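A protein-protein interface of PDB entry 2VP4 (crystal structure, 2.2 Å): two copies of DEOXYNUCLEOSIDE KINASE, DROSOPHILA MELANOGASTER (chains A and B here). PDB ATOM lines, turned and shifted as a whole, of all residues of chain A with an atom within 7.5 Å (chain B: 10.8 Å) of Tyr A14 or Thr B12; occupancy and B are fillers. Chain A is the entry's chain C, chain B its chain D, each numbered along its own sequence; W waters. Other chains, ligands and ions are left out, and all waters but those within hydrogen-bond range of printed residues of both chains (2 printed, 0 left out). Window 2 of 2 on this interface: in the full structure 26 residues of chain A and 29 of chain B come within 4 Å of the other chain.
Along chain B the printed residues that touch a printed residue of chain A span positions 12 to 142. Of the 19 printed residues of chain A, 6 touch a printed residue of chain B. Among the printed residues, 9 pairs touch across the chains. Among the printed residues, no Asp or Glu carboxylate lies within 4 Å of a Lys or Arg side-chain nitrogen of the other chain.
Tyr A14 touches just these residues of chain B: Thr B12, Glu B141 and Ser B142. Of chain A, only Tyr A14 comes within 4 Å of Thr B12. No residue of chain B comes within 4 Å of Ile A143. Of the printed residues of chain B, Thr A12 touches Tyr B14. Of the printed residues of chain B, Ser A142 touches Tyr B14 (3.5 Å). Printed residues of chain A within 4 Å of Tyr B14: Thr A12, Glu A141 and Ser A142. Of the printed residues of chain B, Leu A89 touches Trp B135 (3.5 Å) and Phe B138 (3.9 Å). Gln A19 touches none of the printed residues of chain B. The nearest residue of chain B that does not touch Tyr A14 is Phe B138 (4.2 Å). The nearest printed residue of chain A that does not touch Thr B12 is Ala A15 (4.7 Å). The nearest printed residue of chain B that does not touch Ser A142 is Ile B143 (4.5 Å).
Among the printed residues, merely in contact across the chains: Glu A141 with Tyr B14, Tyr A14 with Glu B141, Thr A12 with Tyr B14, Tyr A14 with Ser B142, Ser A142 with Tyr B14, Leu A89 with Trp B135, Tyr A14 with Thr B12, Thr A93 with Phe B138 and Leu A89 with Phe B138.
O of Leu A89 is in hydrogen-bond range of OG1 of Thr A93 (3.0 Å). N of His B144 lies within hydrogen-bond range of O of Tyr B14 (2.8 Å). The backbone carbonyl oxygen of Thr A93 sits at hydrogen-bond distance from the side-chain amide nitrogen of Gln A19, at 3.5 Å. The backbone NH of Tyr A14 lies within hydrogen-bond range of the backbone carbonyl oxygen of Ser A142 (3.0 Å). O of Ser B142 is in hydrogen-bond range of N of Tyr B14 (2.9 Å). OG of Ser B142 is in hydrogen-bond range of O of Phe B138.
Thr A12 touches Tyr B14, and with the chains exchanged Tyr A14 touches Thr B12. Tyr A14 touches Glu B141, and with the chains exchanged Glu A141 touches Tyr B14. Tyr A14 touches Ser B142, and with the chains exchanged Ser A142 touches Tyr B14.
Water W1 lies within hydrogen-bond range of the backbone carbonyl oxygen (O) of Thr A12 and the backbone NH (N) of Ala B15. Water W2 bridges the backbone carbonyl oxygen (O) of Thr B12 (2.8 Å) and the backbone NH (N) of Ala A15 (2.8 Å).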
ATOM      1  N   THR A  12     -18.842  32.622   6.395  1.00  0.00           N
ATOM      2  CA  THR A  12     -20.262  32.189   6.642  1.00  0.00           C
ATOM      3  C   THR A  12     -20.800  31.351   5.487  1.00  0.00           C
ATOM      4  O   THR A  12     -21.156  31.873   4.431  1.00  0.00           O
ATOM      5  CB  THR A  12     -21.201  33.377   6.861  1.00  0.00           C
ATOM      6  OG1 THR A  12     -20.506  34.402   7.583  1.00  0.00           O
ATOM      7  CG2 THR A  12     -22.448  32.947   7.645  1.00  0.00           C
ATOM      8  N   LYS A  13     -20.869  30.049   5.722  1.00  0.00           N
ATOM      9  CA  LYS A  13     -21.297  29.083   4.720  1.00  0.00           C
ATOM     10  C   LYS A  13     -22.807  28.866   4.724  1.00  0.00           C
ATOM     11  O   LYS A  13     -23.476  29.075   5.736  1.00  0.00           O
ATOM     12  CB  LYS A  13     -20.573  27.762   4.958  1.00  0.00           C
ATOM     13  CG  LYS A  13     -19.068  27.922   5.127  1.00  0.00           C
ATOM     14  CD  LYS A  13     -18.407  26.580   5.249  1.00  0.00           C
ATOM     15  CE  LYS A  13     -17.049  26.709   5.871  1.00  0.00           C
ATOM     16  NZ  LYS A  13     -16.446  25.364   6.018  1.00  0.00           N
ATOM     17  N   TYR A  14     -23.334  28.446   3.575  1.00  0.00           N
ATOM     18  CA  TYR A  14     -24.718  27.983   3.470  1.00  0.00           C
ATOM     19  C   TYR A  14     -24.991  26.845   4.469  1.00  0.00           C
ATOM     20  O   TYR A  14     -24.143  25.966   4.669  1.00  0.00           O
ATOM     21  CB  TYR A  14     -25.003  27.521   2.041  1.00  0.00           C
ATOM     22  CG  TYR A  14     -26.392  26.994   1.810  1.00  0.00           C
ATOM     23  CD1 TYR A  14     -27.497  27.844   1.830  1.00  0.00           C
ATOM     24  CD2 TYR A  14     -26.601  25.646   1.539  1.00  0.00           C
ATOM     25  CE1 TYR A  14     -28.773  27.359   1.608  1.00  0.00           C
ATOM     26  CE2 TYR A  14     -27.870  25.157   1.311  1.00  0.00           C
ATOM     27  CZ  TYR A  14     -28.955  26.014   1.351  1.00  0.00           C
ATOM     28  OH  TYR A  14     -30.222  25.522   1.122  1.00  0.00           O
ATOM     29  N   ALA A  15     -26.166  26.896   5.098  1.00  0.00           N
ATOM     30  CA  ALA A  15     -26.593  25.931   6.127  1.00  0.00           C
ATOM     31  C   ALA A  15     -25.886  26.044   7.489  1.00  0.00           C
ATOM     32  O   ALA A  15     -26.287  25.356   8.434  1.00  0.00           O
ATOM     33  CB  ALA A  15     -26.538  24.481   5.609  1.00  0.00           C
ATOM     34  N   GLU A  16     -24.853  26.892   7.591  1.00  0.00           N
ATOM     35  CA  GLU A  16     -24.161  27.140   8.873  1.00  0.00           C
ATOM     36  C   GLU A  16     -25.129  27.558   9.991  1.00  0.00           C
ATOM     37  O   GLU A  16     -25.929  28.487   9.831  1.00  0.00           O
ATOM     38  CB  GLU A  16     -23.051  28.189   8.715  1.00  0.00           C
ATOM     39  CG  GLU A  16     -21.931  28.055   9.743  1.00  0.00           C
ATOM     40  CD  GLU A  16     -20.817  29.093   9.585  1.00  0.00           C
ATOM     41  OE1 GLU A  16     -20.210  29.198   8.485  1.00  0.00           O
ATOM     42  OE2 GLU A  16     -20.532  29.797  10.587  1.00  0.00           O
ATOM     43  N   GLY A  17     -25.064  26.841  11.109  1.00  0.00           N
ATOM     44  CA  GLY A  17     -25.924  27.111  12.263  1.00  0.00           C
ATOM     45  C   GLY A  17     -27.354  26.600  12.173  1.00  0.00           C
ATOM     46  O   GLY A  17     -28.141  26.808  13.091  1.00  0.00           O
ATOM     47  N   THR A  18     -27.696  25.922  11.081  1.00  0.00           N
ATOM     48  CA  THR A  18     -29.072  25.446  10.872  1.00  0.00           C
ATOM     49  C   THR A  18     -29.255  23.935  11.139  1.00  0.00           C
ATOM     50  O   THR A  18     -30.357  23.404  10.989  1.00  0.00           O
ATOM     51  CB  THR A  18     -29.545  25.733   9.424  1.00  0.00           C
ATOM     52  OG1 THR A  18     -28.787  24.927   8.514  1.00  0.00           O
ATOM     53  CG2 THR A  18     -29.382  27.216   9.056  1.00  0.00           C
ATOM     54  N   GLN A  19     -28.176  23.253  11.521  1.00  0.00           N
ATOM     55  CA  GLN A  19     -28.161  21.790  11.558  1.00  0.00           C
ATOM     56  C   GLN A  19     -28.037  21.204  12.968  1.00  0.00           C
ATOM     57  O   GLN A  19     -27.294  21.735  13.793  1.00  0.00           O
ATOM     58  CB  GLN A  19     -27.026  21.257  10.674  1.00  0.00           C
ATOM     59  CG  GLN A  19     -27.214  21.544   9.178  1.00  0.00           C
ATOM     60  CD  GLN A  19     -28.523  21.004   8.627  1.00  0.00           C
ATOM     61  OE1 GLN A  19     -28.856  19.836   8.815  1.00  0.00           O
ATOM     62  NE2 GLN A  19     -29.265  21.853   7.931  1.00  0.00           N
ATOM     63  N   LEU A  89     -24.706  16.803  -0.666  1.00  0.00           N
ATOM     64  CA  LEU A  89     -24.910  18.206  -0.327  1.00  0.00           C
ATOM     65  C   LEU A  89     -26.349  18.533  -0.045  1.00  0.00           C
ATOM     66  O   LEU A  89     -26.638  19.210   0.951  1.00  0.00           O
ATOM     67  CB  LEU A  89     -24.394  19.106  -1.455  1.00  0.00           C
ATOM     68  CG  LEU A  89     -23.058  19.840  -1.328  1.00  0.00           C
ATOM     69  CD1 LEU A  89     -22.185  19.319  -0.175  1.00  0.00           C
ATOM     70  CD2 LEU A  89     -22.357  19.816  -2.666  1.00  0.00           C
ATOM     71  N   GLN A  90     -27.265  18.095  -0.916  1.00  0.00           N
ATOM     72  CA  GLN A  90     -28.702  18.382  -0.666  1.00  0.00           C
ATOM     73  C   GLN A  90     -29.173  17.799   0.676  1.00  0.00           C
ATOM     74  O   GLN A  90     -29.959  18.413   1.372  1.00  0.00           O
ATOM     75  CB  GLN A  90     -29.615  17.881  -1.787  1.00  0.00           C
ATOM     76  CG  GLN A  90     -29.450  18.578  -3.140  1.00  0.00           C
ATOM     77  CD  GLN A  90     -30.036  17.771  -4.303  1.00  0.00           C
ATOM     78  OE1 GLN A  90     -30.218  16.542  -4.221  1.00  0.00           O
ATOM     79  NE2 GLN A  90     -30.319  18.453  -5.393  1.00  0.00           N
ATOM     80  N   HIS A  92     -27.014  16.798   3.366  1.00  0.00           N
ATOM     81  CA  HIS A  92     -26.256  17.480   4.422  1.00  0.00           C
ATOM     82  C   HIS A  92     -26.874  18.806   4.855  1.00  0.00           C
ATOM     83  O   HIS A  92     -26.859  19.134   6.046  1.00  0.00           O
ATOM     84  CB  HIS A  92     -24.798  17.727   4.022  1.00  0.00           C
ATOM     85  CG  HIS A  92     -23.965  16.489   3.928  1.00  0.00           C
ATOM     86  ND1 HIS A  92     -23.826  15.603   4.974  1.00  0.00           N
ATOM     87  CD2 HIS A  92     -23.201  16.003   2.921  1.00  0.00           C
ATOM     88  CE1 HIS A  92     -23.005  14.628   4.619  1.00  0.00           C
ATOM     89  NE2 HIS A  92     -22.613  14.846   3.379  1.00  0.00           N
ATOM     90  N   THR A  93     -27.399  19.571   3.900  1.00  0.00           N
ATOM     91  CA  THR A  93     -27.896  20.931   4.188  1.00  0.00           C
ATOM     92  C   THR A  93     -29.411  21.051   4.281  1.00  0.00           C
ATOM     93  O   THR A  93     -29.926  22.144   4.532  1.00  0.00           O
ATOM     94  CB  THR A  93     -27.405  21.968   3.144  1.00  0.00           C
ATOM     95  OG1 THR A  93     -28.041  21.723   1.884  1.00  0.00           O
ATOM     96  CG2 THR A  93     -25.909  21.893   2.974  1.00  0.00           C
ATOM     97  N   ALA A  94     -30.127  19.945   4.078  1.00  0.00           N
ATOM     98  CA  ALA A  94     -31.591  19.947   4.191  1.00  0.00           C
ATOM     99  C   ALA A  94     -32.006  20.569   5.527  1.00  0.00           C
ATOM    100  O   ALA A  94     -31.358  20.320   6.548  1.00  0.00           O
ATOM    101  CB  ALA A  94     -32.145  18.528   4.071  1.00  0.00           C
ATOM    102  N   PRO A  95     -33.067  21.404   5.527  1.00  0.00           N
ATOM    103  CA  PRO A  95     -33.487  21.954   6.818  1.00  0.00           C
ATOM    104  C   PRO A  95     -34.275  20.935   7.625  1.00  0.00           C
ATOM    105  O   PRO A  95     -34.882  20.024   7.057  1.00  0.00           O
ATOM    106  CB  PRO A  95     -34.371  23.141   6.422  1.00  0.00           C
ATOM    107  CG  PRO A  95     -34.981  22.714   5.105  1.00  0.00           C
ATOM    108  CD  PRO A  95     -33.903  21.892   4.411  1.00  0.00           C
ATOM    109  N   GLU A 141     -15.107  25.503   1.471  1.00  0.00           N
ATOM    110  CA  GLU A 141     -15.194  26.949   1.733  1.00  0.00           C
ATOM    111  C   GLU A 141     -16.625  27.490   1.790  1.00  0.00           C
ATOM    112  O   GLU A 141     -16.889  28.455   2.496  1.00  0.00           O
ATOM    113  CB  GLU A 141     -14.440  27.757   0.646  1.00  0.00           C
ATOM    114  CG  GLU A 141     -12.994  27.326   0.363  1.00  0.00           C
ATOM    115  CD  GLU A 141     -12.411  27.936  -0.928  1.00  0.00           C
ATOM    116  OE1 GLU A 141     -11.293  27.521  -1.324  1.00  0.00           O
ATOM    117  OE2 GLU A 141     -13.057  28.816  -1.564  1.00  0.00           O
ATOM    118  N   SER A 142     -17.544  26.907   1.029  1.00  0.00           N
ATOM    119  CA  SER A 142     -18.826  27.579   0.814  1.00  0.00           C
ATOM    120  C   SER A 142     -20.037  26.985   1.530  1.00  0.00           C
ATOM    121  O   SER A 142     -21.018  27.687   1.784  1.00  0.00           O
ATOM    122  CB  SER A 142     -19.106  27.737  -0.696  1.00  0.00           C
ATOM    123  OG  SER A 142     -18.996  26.494  -1.371  1.00  0.00           O
ATOM    124  N   ILE A 143     -19.986  25.695   1.842  1.00  0.00           N
ATOM    125  CA  ILE A 143     -21.179  24.993   2.331  1.00  0.00           C
ATOM    126  C   ILE A 143     -20.868  24.255   3.642  1.00  0.00           C
ATOM    127  O   ILE A 143     -19.894  23.505   3.718  1.00  0.00           O
ATOM    128  CB  ILE A 143     -21.710  24.014   1.250  1.00  0.00           C
ATOM    129  CG1 ILE A 143     -22.000  24.770  -0.063  1.00  0.00           C
ATOM    130  CG2 ILE A 143     -22.948  23.237   1.737  1.00  0.00           C
ATOM    131  CD1 ILE A 143     -21.828  23.930  -1.273  1.00  0.00           C
ATOM    132  N   HIS A 144     -21.690  24.487   4.662  1.00  0.00           N
ATOM    133  CA  HIS A 144     -21.534  23.793   5.938  1.00  0.00           C
ATOM    134  C   HIS A 144     -21.982  22.334   5.842  1.00  0.00           C
ATOM    135  O   HIS A 144     -23.132  22.042   5.464  1.00  0.00           O
ATOM    136  CB  HIS A 144     -22.296  24.507   7.069  1.00  0.00           C
ATOM    137  CG  HIS A 144     -22.179  23.819   8.392  1.00  0.00           C
ATOM    138  ND1 HIS A 144     -20.986  23.725   9.078  1.00  0.00           N
ATOM    139  CD2 HIS A 144     -23.095  23.155   9.137  1.00  0.00           C
ATOM    140  CE1 HIS A 144     -21.176  23.044  10.195  1.00  0.00           C
ATOM    141  NE2 HIS A 144     -22.449  22.689  10.256  1.00  0.00           N
ATOM    142  N   VAL A 145     -21.059  21.438   6.168  1.00  0.00           N
ATOM    143  CA  VAL A 145     -21.328  20.006   6.264  1.00  0.00           C
ATOM    144  C   VAL A 145     -21.187  19.514   7.730  1.00  0.00           C
ATOM    145  O   VAL A 145     -20.091  19.206   8.208  1.00  0.00           O
ATOM    146  CB  VAL A 145     -20.459  19.180   5.270  1.00  0.00           C
ATOM    147  CG1 VAL A 145     -20.764  17.711   5.394  1.00  0.00           C
ATOM    148  CG2 VAL A 145     -20.734  19.620   3.824  1.00  0.00           C
ATOM    149  N   THR B  12     -29.490  32.023   4.774  1.00  0.00           N
ATOM    150  CA  THR B  12     -28.655  32.974   3.969  1.00  0.00           C
ATOM    151  C   THR B  12     -27.590  32.234   3.148  1.00  0.00           C
ATOM    152  O   THR B  12     -27.027  31.224   3.599  1.00  0.00           O
ATOM    153  CB  THR B  12     -27.938  34.017   4.853  1.00  0.00           C
ATOM    154  OG1 THR B  12     -27.158  33.340   5.847  1.00  0.00           O
ATOM    155  CG2 THR B  12     -28.933  34.965   5.522  1.00  0.00           C
ATOM    156  N   LYS B  13     -27.306  32.747   1.954  1.00  0.00           N
ATOM    157  CA  LYS B  13     -26.435  32.060   1.023  1.00  0.00           C
ATOM    158  C   LYS B  13     -24.980  32.430   1.263  1.00  0.00           C
ATOM    159  O   LYS B  13     -24.682  33.464   1.861  1.00  0.00           O
ATOM    160  CB  LYS B  13     -26.857  32.379  -0.406  1.00  0.00           C
ATOM    161  CG  LYS B  13     -28.322  32.129  -0.642  1.00  0.00           C
ATOM    162  CD  LYS B  13     -28.769  32.497  -2.039  1.00  0.00           C
ATOM    163  CE  LYS B  13     -30.274  32.713  -2.034  1.00  0.00           C
ATOM    164  NZ  LYS B  13     -30.989  32.178  -3.235  1.00  0.00           N
ATOM    165  N   TYR B  14     -24.069  31.581   0.803  1.00  0.00           N
ATOM    166  CA  TYR B  14     -22.666  31.931   0.819  1.00  0.00           C
ATOM    167  C   TYR B  14     -22.379  33.187  -0.035  1.00  0.00           C
ATOM    168  O   TYR B  14     -22.860  33.306  -1.171  1.00  0.00           O
ATOM    169  CB  TYR B  14     -21.832  30.746   0.366  1.00  0.00           C
ATOM    170  CG  TYR B  14     -20.352  31.010   0.312  1.00  0.00           C
ATOM    171  CD1 TYR B  14     -19.605  31.087   1.479  1.00  0.00           C
ATOM    172  CD2 TYR B  14     -19.694  31.173  -0.908  1.00  0.00           C
ATOM    173  CE1 TYR B  14     -18.257  31.323   1.442  1.00  0.00           C
ATOM    174  CE2 TYR B  14     -18.337  31.409  -0.953  1.00  0.00           C
ATOM    175  CZ  TYR B  14     -17.625  31.486   0.228  1.00  0.00           C
ATOM    176  OH  TYR B  14     -16.268  31.718   0.213  1.00  0.00           O
ATOM    177  N   ALA B  15     -21.619  34.117   0.556  1.00  0.00           N
ATOM    178  CA  ALA B  15     -21.217  35.397  -0.058  1.00  0.00           C
ATOM    179  C   ALA B  15     -22.296  36.490   0.007  1.00  0.00           C
ATOM    180  O   ALA B  15     -22.065  37.629  -0.417  1.00  0.00           O
ATOM    181  CB  ALA B  15     -20.692  35.200  -1.507  1.00  0.00           C
ATOM    182  N   GLU B  16     -23.455  36.150   0.563  1.00  0.00           N
ATOM    183  CA  GLU B  16     -24.543  37.104   0.737  1.00  0.00           C
ATOM    184  C   GLU B  16     -24.121  38.272   1.626  1.00  0.00           C
ATOM    185  O   GLU B  16     -23.555  38.069   2.694  1.00  0.00           O
ATOM    186  CB  GLU B  16     -25.784  36.421   1.317  1.00  0.00           C
ATOM    187  CG  GLU B  16     -27.023  37.307   1.334  1.00  0.00           C
ATOM    188  CD  GLU B  16     -28.309  36.527   1.142  1.00  0.00           C
ATOM    189  OE1 GLU B  16     -28.630  35.670   1.995  1.00  0.00           O
ATOM    190  OE2 GLU B  16     -29.002  36.782   0.128  1.00  0.00           O
ATOM    191  N   GLY B  17     -24.373  39.491   1.154  1.00  0.00           N
ATOM    192  CA  GLY B  17     -24.022  40.704   1.899  1.00  0.00           C
ATOM    193  C   GLY B  17     -22.539  41.045   1.883  1.00  0.00           C
ATOM    194  O   GLY B  17     -22.117  42.000   2.548  1.00  0.00           O
ATOM    195  N   THR B  18     -21.746  40.286   1.124  1.00  0.00           N
ATOM    196  CA  THR B  18     -20.294  40.497   1.079  1.00  0.00           C
ATOM    197  C   THR B  18     -19.823  41.153  -0.227  1.00  0.00           C
ATOM    198  O   THR B  18     -18.621  41.390  -0.418  1.00  0.00           O
ATOM    199  CB  THR B  18     -19.494  39.161   1.290  1.00  0.00           C
ATOM    200  OG1 THR B  18     -19.384  38.448   0.051  1.00  0.00           O
ATOM    201  CG2 THR B  18     -20.140  38.267   2.354  1.00  0.00           C
ATOM    202  N   THR B  93     -17.879  34.857  -5.943  1.00  0.00           N
ATOM    203  CA  THR B  93     -17.917  34.892  -4.481  1.00  0.00           C
ATOM    204  C   THR B  93     -16.643  35.448  -3.898  1.00  0.00           C
ATOM    205  O   THR B  93     -16.522  35.583  -2.675  1.00  0.00           O
ATOM    206  CB  THR B  93     -18.138  33.502  -3.867  1.00  0.00           C
ATOM    207  OG1 THR B  93     -17.040  32.642  -4.209  1.00  0.00           O
ATOM    208  CG2 THR B  93     -19.464  32.920  -4.310  1.00  0.00           C
ATOM    209  N   TRP B 135     -27.300  20.762 -10.486  1.00  0.00           N
ATOM    210  CA  TRP B 135     -26.289  21.598  -9.831  1.00  0.00           C
ATOM    211  C   TRP B 135     -26.642  23.098  -9.836  1.00  0.00           C
ATOM    212  O   TRP B 135     -26.557  23.761  -8.819  1.00  0.00           O
ATOM    213  CB  TRP B 135     -24.912  21.368 -10.439  1.00  0.00           C
ATOM    214  CG  TRP B 135     -24.099  20.407  -9.656  1.00  0.00           C
ATOM    215  CD1 TRP B 135     -23.848  19.088  -9.965  1.00  0.00           C
ATOM    216  CD2 TRP B 135     -23.432  20.660  -8.414  1.00  0.00           C
ATOM    217  NE1 TRP B 135     -23.067  18.514  -8.989  1.00  0.00           N
ATOM    218  CE2 TRP B 135     -22.790  19.455  -8.030  1.00  0.00           C
ATOM    219  CE3 TRP B 135     -23.314  21.786  -7.586  1.00  0.00           C
ATOM    220  CZ2 TRP B 135     -22.025  19.352  -6.848  1.00  0.00           C
ATOM    221  CZ3 TRP B 135     -22.558  21.678  -6.411  1.00  0.00           C
ATOM    222  CH2 TRP B 135     -21.917  20.469  -6.064  1.00  0.00           C
ATOM    223  N   LYS B 137     -29.580  24.531  -9.993  1.00  0.00           N
ATOM    224  CA  LYS B 137     -30.717  24.799  -9.114  1.00  0.00           C
ATOM    225  C   LYS B 137     -30.251  24.878  -7.667  1.00  0.00           C
ATOM    226  O   LYS B 137     -30.669  25.766  -6.932  1.00  0.00           O
ATOM    227  CB  LYS B 137     -31.811  23.735  -9.273  1.00  0.00           C
ATOM    228  CG  LYS B 137     -32.497  23.785 -10.629  1.00  0.00           C
ATOM    229  CD  LYS B 137     -33.286  22.503 -10.889  1.00  0.00           C
ATOM    230  CE  LYS B 137     -33.649  22.374 -12.371  1.00  0.00           C
ATOM    231  NZ  LYS B 137     -34.742  21.365 -12.596  1.00  0.00           N
ATOM    232  N   PHE B 138     -29.395  23.944  -7.268  1.00  0.00           N
ATOM    233  CA  PHE B 138     -28.810  23.972  -5.921  1.00  0.00           C
ATOM    234  C   PHE B 138     -27.870  25.163  -5.688  1.00  0.00           C
ATOM    235  O   PHE B 138     -27.841  25.716  -4.596  1.00  0.00           O
ATOM    236  CB  PHE B 138     -28.098  22.650  -5.602  1.00  0.00           C
ATOM    237  CG  PHE B 138     -27.388  22.645  -4.277  1.00  0.00           C
ATOM    238  CD1 PHE B 138     -28.101  22.463  -3.089  1.00  0.00           C
ATOM    239  CD2 PHE B 138     -26.004  22.819  -4.219  1.00  0.00           C
ATOM    240  CE1 PHE B 138     -27.447  22.476  -1.844  1.00  0.00           C
ATOM    241  CE2 PHE B 138     -25.334  22.830  -2.995  1.00  0.00           C
ATOM    242  CZ  PHE B 138     -26.061  22.657  -1.793  1.00  0.00           C
ATOM    243  N   ILE B 139     -27.086  25.541  -6.695  1.00  0.00           N
ATOM    244  CA  ILE B 139     -26.243  26.755  -6.591  1.00  0.00           C
ATOM    245  C   ILE B 139     -27.109  28.004  -6.343  1.00  0.00           C
ATOM    246  O   ILE B 139     -26.783  28.816  -5.490  1.00  0.00           O
ATOM    247  CB  ILE B 139     -25.318  26.929  -7.843  1.00  0.00           C
ATOM    248  CG1 ILE B 139     -24.228  25.853  -7.854  1.00  0.00           C
ATOM    249  CG2 ILE B 139     -24.663  28.321  -7.880  1.00  0.00           C
ATOM    250  CD1 ILE B 139     -23.723  25.466  -9.252  1.00  0.00           C
ATOM    251  N   GLU B 140     -28.221  28.136  -7.063  1.00  0.00           N
ATOM    252  CA  GLU B 140     -29.205  29.208  -6.818  1.00  0.00           C
ATOM    253  C   GLU B 140     -29.645  29.325  -5.360  1.00  0.00           C
ATOM    254  O   GLU B 140     -29.838  30.428  -4.857  1.00  0.00           O
ATOM    255  CB  GLU B 140     -30.471  28.998  -7.641  1.00  0.00           C
ATOM    256  CG  GLU B 140     -30.348  29.272  -9.110  1.00  0.00           C
ATOM    257  CD  GLU B 140     -31.709  29.488  -9.762  1.00  0.00           C
ATOM    258  OE1 GLU B 140     -32.273  30.597  -9.587  1.00  0.00           O
ATOM    259  OE2 GLU B 140     -32.210  28.553 -10.447  1.00  0.00           O
ATOM    260  N   GLU B 141     -29.831  28.183  -4.704  1.00  0.00           N
ATOM    261  CA  GLU B 141     -30.291  28.141  -3.325  1.00  0.00           C
ATOM    262  C   GLU B 141     -29.181  28.458  -2.324  1.00  0.00           C
ATOM    263  O   GLU B 141     -29.437  29.055  -1.281  1.00  0.00           O
ATOM    264  CB  GLU B 141     -30.879  26.765  -3.018  1.00  0.00           C
ATOM    265  CG  GLU B 141     -32.083  26.386  -3.895  1.00  0.00           C
ATOM    266  CD  GLU B 141     -32.549  24.924  -3.700  1.00  0.00           C
ATOM    267  OE1 GLU B 141     -33.632  24.574  -4.237  1.00  0.00           O
ATOM    268  OE2 GLU B 141     -31.849  24.129  -3.021  1.00  0.00           O
ATOM    269  N   SER B 142     -27.950  28.082  -2.656  1.00  0.00           N
ATOM    270  CA  SER B 142     -26.867  28.037  -1.675  1.00  0.00           C
ATOM    271  C   SER B 142     -25.806  29.116  -1.822  1.00  0.00           C
ATOM    272  O   SER B 142     -25.093  29.411  -0.862  1.00  0.00           O
ATOM    273  CB  SER B 142     -26.179  26.673  -1.745  1.00  0.00           C
ATOM    274  OG  SER B 142     -25.593  26.447  -3.017  1.00  0.00           O
ATOM    275  N   ILE B 143     -25.676  29.682  -3.021  1.00  0.00           N
ATOM    276  CA  ILE B 143     -24.589  30.610  -3.317  1.00  0.00           C
ATOM    277  C   ILE B 143     -25.096  31.935  -3.915  1.00  0.00           C
ATOM    278  O   ILE B 143     -25.809  31.966  -4.925  1.00  0.00           O
ATOM    279  CB  ILE B 143     -23.477  29.918  -4.171  1.00  0.00           C
ATOM    280  CG1 ILE B 143     -22.768  28.845  -3.330  1.00  0.00           C
ATOM    281  CG2 ILE B 143     -22.452  30.921  -4.673  1.00  0.00           C
ATOM    282  CD1 ILE B 143     -22.337  27.662  -4.111  1.00  0.00           C
ATOM    283  N   HIS B 144     -24.769  33.032  -3.234  1.00  0.00           N
ATOM    284  CA  HIS B 144     -25.157  34.362  -3.700  1.00  0.00           C
ATOM    285  C   HIS B 144     -24.330  34.803  -4.922  1.00  0.00           C
ATOM    286  O   HIS B 144     -23.097  34.824  -4.882  1.00  0.00           O
ATOM    287  CB  HIS B 144     -25.039  35.368  -2.558  1.00  0.00           C
ATOM    288  CG  HIS B 144     -25.226  36.785  -2.980  1.00  0.00           C
ATOM    289  ND1 HIS B 144     -26.455  37.295  -3.348  1.00  0.00           N
ATOM    290  CD2 HIS B 144     -24.342  37.807  -3.084  1.00  0.00           C
ATOM    291  CE1 HIS B 144     -26.318  38.569  -3.664  1.00  0.00           C
ATOM    292  NE2 HIS B 144     -25.047  38.904  -3.513  1.00  0.00           N
ATOM    293  N   VAL B 145     -25.026  35.131  -6.005  1.00  0.00           N
ATOM    294  CA  VAL B 145     -24.387  35.622  -7.215  1.00  0.00           C
ATOM    295  C   VAL B 145     -24.841  37.064  -7.457  1.00  0.00           C
ATOM    296  O   VAL B 145     -25.970  37.322  -7.879  1.00  0.00           O
ATOM    297  CB  VAL B 145     -24.653  34.705  -8.453  1.00  0.00           C
ATOM    298  CG1 VAL B 145     -23.955  35.257  -9.674  1.00  0.00           C
ATOM    299  CG2 VAL B 145     -24.156  33.287  -8.196  1.00  0.00           C
HETATM  300  O   HOH W   1     -20.620  34.050   3.062  1.00  0.00           O
HETATM  301  O   HOH W   2     -27.792  29.215   5.333  1.00  0.00           O
